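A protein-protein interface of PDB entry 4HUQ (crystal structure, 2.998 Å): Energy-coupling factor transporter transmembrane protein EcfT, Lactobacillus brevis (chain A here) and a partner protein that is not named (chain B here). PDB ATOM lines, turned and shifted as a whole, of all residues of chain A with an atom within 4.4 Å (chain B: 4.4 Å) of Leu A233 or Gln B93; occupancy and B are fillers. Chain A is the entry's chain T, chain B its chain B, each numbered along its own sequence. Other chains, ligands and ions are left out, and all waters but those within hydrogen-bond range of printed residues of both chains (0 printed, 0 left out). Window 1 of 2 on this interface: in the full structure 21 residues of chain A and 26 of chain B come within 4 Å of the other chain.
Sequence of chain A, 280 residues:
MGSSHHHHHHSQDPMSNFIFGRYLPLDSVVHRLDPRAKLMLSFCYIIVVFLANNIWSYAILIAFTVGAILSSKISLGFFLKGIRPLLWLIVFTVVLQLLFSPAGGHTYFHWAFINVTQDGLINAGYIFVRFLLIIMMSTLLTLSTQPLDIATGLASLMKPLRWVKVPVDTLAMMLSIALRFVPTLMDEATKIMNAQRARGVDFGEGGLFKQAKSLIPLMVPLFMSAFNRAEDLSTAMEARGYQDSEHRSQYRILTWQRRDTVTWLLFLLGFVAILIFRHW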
ATOM      1  N   ILE A 177     -13.187 -10.084 -31.293  1.00  0.00           N
ATOM      2  CA  ILE A 177     -14.201 -10.941 -30.717  1.00  0.00           C
ATOM      3  C   ILE A 177     -14.311 -12.214 -31.553  1.00  0.00           C
ATOM      4  O   ILE A 177     -14.201 -13.320 -31.026  1.00  0.00           O
ATOM      5  CB  ILE A 177     -15.568 -10.228 -30.635  1.00  0.00           C
ATOM      6  CG1 ILE A 177     -15.733  -9.548 -29.273  1.00  0.00           C
ATOM      7  CG2 ILE A 177     -16.726 -11.210 -30.847  1.00  0.00           C
ATOM      8  CD1 ILE A 177     -15.257  -8.126 -29.230  1.00  0.00           C
ATOM      9  N   PHE A 181     -13.591 -16.205 -30.056  1.00  0.00           N
ATOM     10  CA  PHE A 181     -14.677 -17.179 -30.008  1.00  0.00           C
ATOM     11  C   PHE A 181     -14.490 -18.424 -30.881  1.00  0.00           C
ATOM     12  O   PHE A 181     -15.042 -19.483 -30.579  1.00  0.00           O
ATOM     13  CB  PHE A 181     -15.995 -16.512 -30.356  1.00  0.00           C
ATOM     14  CG  PHE A 181     -16.657 -15.897 -29.185  1.00  0.00           C
ATOM     15  CD1 PHE A 181     -16.427 -16.400 -27.922  1.00  0.00           C
ATOM     16  CD2 PHE A 181     -17.487 -14.803 -29.334  1.00  0.00           C
ATOM     17  CE1 PHE A 181     -17.018 -15.837 -26.835  1.00  0.00           C
ATOM     18  CE2 PHE A 181     -18.085 -14.233 -28.247  1.00  0.00           C
ATOM     19  CZ  PHE A 181     -17.851 -14.748 -26.994  1.00  0.00           C
ATOM     20  N   ARG A 229     -23.647 -16.611 -25.257  1.00  0.00           N
ATOM     21  CA  ARG A 229     -22.285 -16.146 -25.000  1.00  0.00           C
ATOM     22  C   ARG A 229     -22.107 -14.691 -25.391  1.00  0.00           C
ATOM     23  O   ARG A 229     -21.464 -13.930 -24.673  1.00  0.00           O
ATOM     24  CB  ARG A 229     -21.253 -17.034 -25.705  1.00  0.00           C
ATOM     25  CG  ARG A 229     -21.084 -18.367 -25.022  1.00  0.00           C
ATOM     26  CD  ARG A 229     -20.307 -19.387 -25.834  1.00  0.00           C
ATOM     27  NE  ARG A 229     -20.607 -20.709 -25.311  1.00  0.00           N
ATOM     28  CZ  ARG A 229     -20.071 -21.220 -24.207  1.00  0.00           C
ATOM     29  NH1 ARG A 229     -19.170 -20.531 -23.523  1.00  0.00           N
ATOM     30  NH2 ARG A 229     -20.437 -22.431 -23.795  1.00  0.00           N
ATOM     31  N   ALA A 230     -22.689 -14.310 -26.525  1.00  0.00           N
ATOM     32  CA  ALA A 230     -22.645 -12.921 -26.977  1.00  0.00           C
ATOM     33  C   ALA A 230     -23.153 -11.997 -25.895  1.00  0.00           C
ATOM     34  O   ALA A 230     -22.447 -11.080 -25.481  1.00  0.00           O
ATOM     35  CB  ALA A 230     -23.462 -12.731 -28.245  1.00  0.00           C
ATOM     36  N   GLU A 231     -24.376 -12.257 -25.439  1.00  0.00           N
ATOM     37  CA  GLU A 231     -25.039 -11.376 -24.487  1.00  0.00           C
ATOM     38  C   GLU A 231     -24.199 -11.241 -23.234  1.00  0.00           C
ATOM     39  O   GLU A 231     -23.865 -10.131 -22.833  1.00  0.00           O
ATOM     40  CB  GLU A 231     -26.446 -11.872 -24.144  1.00  0.00           C
ATOM     41  CG  GLU A 231     -27.240 -10.899 -23.281  1.00  0.00           C
ATOM     42  CD  GLU A 231     -28.723 -10.928 -23.596  1.00  0.00           C
ATOM     43  OE1 GLU A 231     -29.145 -11.820 -24.362  1.00  0.00           O
ATOM     44  OE2 GLU A 231     -29.464 -10.058 -23.087  1.00  0.00           O
ATOM     45  N   ASP A 232     -23.830 -12.380 -22.654  1.00  0.00           N
ATOM     46  CA  ASP A 232     -23.000 -12.406 -21.456  1.00  0.00           C
ATOM     47  C   ASP A 232     -21.718 -11.592 -21.644  1.00  0.00           C
ATOM     48  O   ASP A 232     -21.299 -10.870 -20.747  1.00  0.00           O
ATOM     49  CB  ASP A 232     -22.674 -13.849 -21.025  1.00  0.00           C
ATOM     50  CG  ASP A 232     -23.832 -14.528 -20.287  1.00  0.00           C
ATOM     51  OD1 ASP A 232     -25.003 -14.275 -20.641  1.00  0.00           O
ATOM     52  OD2 ASP A 232     -23.568 -15.324 -19.353  1.00  0.00           O
ATOM     53  N   LEU A 233     -21.105 -11.685 -22.815  1.00  0.00           N
ATOM     54  CA  LEU A 233     -19.855 -10.963 -23.035  1.00  0.00           C
ATOM     55  C   LEU A 233     -20.056  -9.456 -23.142  1.00  0.00           C
ATOM     56  O   LEU A 233     -19.273  -8.677 -22.607  1.00  0.00           O
ATOM     57  CB  LEU A 233     -19.131 -11.473 -24.273  1.00  0.00           C
ATOM     58  CG  LEU A 233     -17.885 -10.654 -24.633  1.00  0.00           C
ATOM     59  CD1 LEU A 233     -16.820 -10.713 -23.540  1.00  0.00           C
ATOM     60  CD2 LEU A 233     -17.318 -11.086 -25.972  1.00  0.00           C
ATOM     61  N   SER A 234     -21.106  -9.054 -23.845  1.00  0.00           N
ATOM     62  CA  SER A 234     -21.384  -7.648 -24.064  1.00  0.00           C
ATOM     63  C   SER A 234     -21.604  -6.929 -22.736  1.00  0.00           C
ATOM     64  O   SER A 234     -20.995  -5.887 -22.482  1.00  0.00           O
ATOM     65  CB  SER A 234     -22.618  -7.503 -24.948  1.00  0.00           C
ATOM     66  OG  SER A 234     -23.294  -6.299 -24.661  1.00  0.00           O
ATOM     67  N   THR A 235     -22.468  -7.493 -21.888  1.00  0.00           N
ATOM     68  CA  THR A 235     -22.760  -6.880 -20.595  1.00  0.00           C
ATOM     69  C   THR A 235     -21.481  -6.742 -19.787  1.00  0.00           C
ATOM     70  O   THR A 235     -21.198  -5.679 -19.233  1.00  0.00           O
ATOM     71  CB  THR A 235     -23.859  -7.635 -19.791  1.00  0.00           C
ATOM     72  OG1 THR A 235     -23.657  -7.450 -18.379  1.00  0.00           O
ATOM     73  CG2 THR A 235     -23.801  -9.082 -20.074  1.00  0.00           C
ATOM     74  N   ALA A 236     -20.688  -7.805 -19.768  1.00  0.00           N
ATOM     75  CA  ALA A 236     -19.437  -7.817 -19.028  1.00  0.00           C
ATOM     76  C   ALA A 236     -18.509  -6.749 -19.579  1.00  0.00           C
ATOM     77  O   ALA A 236     -17.790  -6.092 -18.830  1.00  0.00           O
ATOM     78  CB  ALA A 236     -18.783  -9.186 -19.111  1.00  0.00           C
ATOM     79  N   MET A 237     -18.518  -6.586 -20.897  1.00  0.00           N
ATOM     80  CA  MET A 237     -17.705  -5.561 -21.534  1.00  0.00           C
ATOM     81  C   MET A 237     -18.147  -4.187 -21.055  1.00  0.00           C
ATOM     82  O   MET A 237     -17.320  -3.322 -20.789  1.00  0.00           O
ATOM     83  CB  MET A 237     -17.839  -5.645 -23.053  1.00  0.00           C
ATOM     84  CG  MET A 237     -16.774  -6.491 -23.725  1.00  0.00           C
ATOM     85  SD  MET A 237     -16.943  -6.473 -25.516  1.00  0.00           S
ATOM     86  CE  MET A 237     -18.395  -5.444 -25.705  1.00  0.00           C
ATOM     87  N   MET B  85     -17.005  -5.679 -11.425  1.00  0.00           N
ATOM     88  CA  MET B  85     -17.979  -6.747 -11.296  1.00  0.00           C
ATOM     89  C   MET B  85     -17.508  -8.078 -11.911  1.00  0.00           C
ATOM     90  O   MET B  85     -17.400  -8.208 -13.125  1.00  0.00           O
ATOM     91  CB  MET B  85     -19.293  -6.286 -11.933  1.00  0.00           C
ATOM     92  CG  MET B  85     -20.521  -7.012 -11.421  1.00  0.00           C
ATOM     93  SD  MET B  85     -22.051  -6.227 -11.927  1.00  0.00           S
ATOM     94  CE  MET B  85     -23.254  -7.320 -11.179  1.00  0.00           C
ATOM     95  N   ILE B  86     -17.228  -9.069 -11.073  1.00  0.00           N
ATOM     96  CA  ILE B  86     -16.957 -10.425 -11.565  1.00  0.00           C
ATOM     97  C   ILE B  86     -18.270 -11.180 -11.724  1.00  0.00           C
ATOM     98  O   ILE B  86     -19.058 -11.258 -10.790  1.00  0.00           O
ATOM     99  CB  ILE B  86     -16.048 -11.242 -10.601  1.00  0.00           C
ATOM    100  CG1 ILE B  86     -14.839 -10.425 -10.146  1.00  0.00           C
ATOM    101  CG2 ILE B  86     -15.598 -12.552 -11.252  1.00  0.00           C
ATOM    102  CD1 ILE B  86     -13.937 -10.071 -11.255  1.00  0.00           C
ATOM    103  N   PHE B  87     -18.495 -11.757 -12.894  1.00  0.00           N
ATOM    104  CA  PHE B  87     -19.770 -12.409 -13.174  1.00  0.00           C
ATOM    105  C   PHE B  87     -19.737 -13.927 -12.947  1.00  0.00           C
ATOM    106  O   PHE B  87     -18.669 -14.521 -12.778  1.00  0.00           O
ATOM    107  CB  PHE B  87     -20.208 -12.080 -14.597  1.00  0.00           C
ATOM    108  CG  PHE B  87     -20.481 -10.610 -14.831  1.00  0.00           C
ATOM    109  CD1 PHE B  87     -19.447  -9.714 -15.036  1.00  0.00           C
ATOM    110  CD2 PHE B  87     -21.777 -10.133 -14.864  1.00  0.00           C
ATOM    111  CE1 PHE B  87     -19.705  -8.377 -15.268  1.00  0.00           C
ATOM    112  CE2 PHE B  87     -22.044  -8.792 -15.088  1.00  0.00           C
ATOM    113  CZ  PHE B  87     -21.010  -7.917 -15.293  1.00  0.00           C
ATOM    114  N   ASN B  89     -20.139 -17.707 -14.292  1.00  0.00           N
ATOM    115  CA  ASN B  89     -19.768 -18.251 -15.617  1.00  0.00           C
ATOM    116  C   ASN B  89     -18.541 -17.589 -16.207  1.00  0.00           C
ATOM    117  O   ASN B  89     -18.644 -16.601 -16.923  1.00  0.00           O
ATOM    118  CB  ASN B  89     -20.926 -18.191 -16.635  1.00  0.00           C
ATOM    119  CG  ASN B  89     -20.646 -18.992 -17.906  1.00  0.00           C
ATOM    120  OD1 ASN B  89     -19.511 -19.061 -18.390  1.00  0.00           O
ATOM    121  ND2 ASN B  89     -21.696 -19.618 -18.441  1.00  0.00           N
ATOM    122  N   ASN B  92     -17.349 -17.176 -20.306  1.00  0.00           N
ATOM    123  CA  ASN B  92     -17.664 -15.916 -20.988  1.00  0.00           C
ATOM    124  C   ASN B  92     -16.922 -14.732 -20.364  1.00  0.00           C
ATOM    125  O   ASN B  92     -15.851 -14.915 -19.774  1.00  0.00           O
ATOM    126  CB  ASN B  92     -19.173 -15.662 -20.990  1.00  0.00           C
ATOM    127  CG  ASN B  92     -19.971 -16.889 -21.417  1.00  0.00           C
ATOM    128  OD1 ASN B  92     -19.466 -17.755 -22.131  1.00  0.00           O
ATOM    129  ND2 ASN B  92     -21.221 -16.967 -20.977  1.00  0.00           N
ATOM    130  N   GLN B  93     -17.484 -13.528 -20.500  1.00  0.00           N
ATOM    131  CA  GLN B  93     -16.910 -12.281 -19.914  1.00  0.00           C
ATOM    132  C   GLN B  93     -15.402 -11.993 -20.128  1.00  0.00           C
ATOM    133  O   GLN B  93     -14.765 -11.347 -19.299  1.00  0.00           O
ATOM    134  CB  GLN B  93     -17.309 -12.096 -18.423  1.00  0.00           C
ATOM    135  CG  GLN B  93     -16.520 -12.875 -17.367  1.00  0.00           C
ATOM    136  CD  GLN B  93     -16.806 -12.398 -15.938  1.00  0.00           C
ATOM    137  OE1 GLN B  93     -16.944 -11.202 -15.682  1.00  0.00           O
ATOM    138  NE2 GLN B  93     -16.879 -13.335 -15.006  1.00  0.00           N
ATOM    139  N   PHE B  94     -14.849 -12.429 -21.262  1.00  0.00           N
ATOM    140  CA  PHE B  94     -13.407 -12.328 -21.489  1.00  0.00           C
ATOM    141  C   PHE B  94     -12.956 -11.148 -22.331  1.00  0.00           C
ATOM    142  O   PHE B  94     -12.433 -10.185 -21.779  1.00  0.00           O
ATOM    143  CB  PHE B  94     -12.842 -13.618 -22.069  1.00  0.00           C
ATOM    144  CG  PHE B  94     -11.497 -13.982 -21.517  1.00  0.00           C
ATOM    145  CD1 PHE B  94     -11.383 -14.614 -20.290  1.00  0.00           C
ATOM    146  CD2 PHE B  94     -10.343 -13.691 -22.222  1.00  0.00           C
ATOM    147  CE1 PHE B  94     -10.138 -14.953 -19.778  1.00  0.00           C
ATOM    148  CE2 PHE B  94      -9.094 -14.026 -21.717  1.00  0.00           C
ATOM    149  CZ  PHE B  94      -8.993 -14.660 -20.493  1.00  0.00           C
ATOM    150  N   VAL B  95     -13.183 -11.216 -23.646  1.00  0.00           N
ATOM    151  CA  VAL B  95     -12.473 -10.374 -24.652  1.00  0.00           C
ATOM    152  C   VAL B  95     -10.954 -10.314 -24.475  1.00  0.00           C
ATOM    153  O   VAL B  95     -10.431  -9.857 -23.456  1.00  0.00           O
ATOM    154  CB  VAL B  95     -13.067  -8.918 -24.915  1.00  0.00           C
ATOM    155  CG1 VAL B  95     -14.420  -8.996 -25.604  1.00  0.00           C
ATOM    156  CG2 VAL B  95     -13.113  -8.034 -23.660  1.00  0.00           C
ATOM    157  N   GLN B 147     -11.311 -16.648 -13.855  1.00  0.00           N
ATOM    158  CA  GLN B 147     -11.925 -15.736 -12.902  1.00  0.00           C
ATOM    159  C   GLN B 147     -10.909 -14.776 -12.314  1.00  0.00           C
ATOM    160  O   GLN B 147     -11.172 -13.586 -12.180  1.00  0.00           O
ATOM    161  CB  GLN B 147     -12.602 -16.524 -11.797  1.00  0.00           C
ATOM    162  CG  GLN B 147     -13.924 -15.942 -11.382  1.00  0.00           C
ATOM    163  CD  GLN B 147     -15.037 -16.175 -12.378  1.00  0.00           C
ATOM    164  OE1 GLN B 147     -14.957 -15.775 -13.536  1.00  0.00           O
ATOM    165  NE2 GLN B 147     -16.107 -16.796 -11.914  1.00  0.00           N
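OD1 of Asn B92 lies within hydrogen-bond range of NH1 of Arg A229, 3.1 Å away.
ND2 of Asn B92 sits at hydrogen-bond distance from OD2 of Asp A232 (3.3 Å).
N of Phe B87 lies close to NE2 of Gln B93 (3.1 Å).
The backbone NH (N) of Asn B92 lies within hydrogen-bond range of the side-chain amide oxygen (OD1) of Asn B89 (3.4 Å).
OE1 of Gln B147 sits at hydrogen-bond distance from NE2 of Gln B93, 3.4 Å away.
Among the printed residues, merely in contact across the chains: Ala A236 with Gln B93, Leu A233 with Phe B94, Met A237 with Val B95, Leu A233 with Val B95, Ala A236 with Phe B87, Ile A177 with Val B95, Thr A235 with Phe B87 and Leu A233 with Gln B93.
Of the printed residues of chain B, Ile A177 touches Val B95 (3.8 Å).
Of the printed residues of chain B, Arg A229 touches Asn B92.
Leu A233 touches just these residues of chain B: Gln B93 (3.9 Å), Phe B94 (3.5 Å) and Val B95 (3.6 Å).
Ser A234 touches none of the printed residues of chain B.
Of the printed residues of chain B, Met A237 touches Val B95 (3.6 Å).
Printed residues of chain A within 4 Å of Phe B87: Thr A235 and Ala A236.
Asn B89 touches none of the printed residues of chain A.
Of the printed residues of chain A, Asn B92 touches Arg A229 (3.1 Å) and Asp A232 (3.3 Å).
Gln B93 touches just these residues of chain A: Leu A233 and Ala A236.
The nearest printed residue of chain B that does not touch Leu A233 is Asn B92 (4.8 Å).
The nearest printed residue of chain A that does not touch Val B95 is Phe A181 (6.7 Å).
Of the 11 printed residues of chain A, 7 touch a printed residue of chain B.
Hydrophobic or aromatic side chains of chain A within 4 Å of the printed part of chain B: Ile A177, Leu A233, Ala A236 and Met A237.
Of the 9 printed residues of chain B, 5 touch a printed residue of chain A.
Hydrophobic or aromatic side chains of chain B that line the printed part of chain A: Phe B87 and Val B95.
Among the printed residues, 10 pairs touch across the chains.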
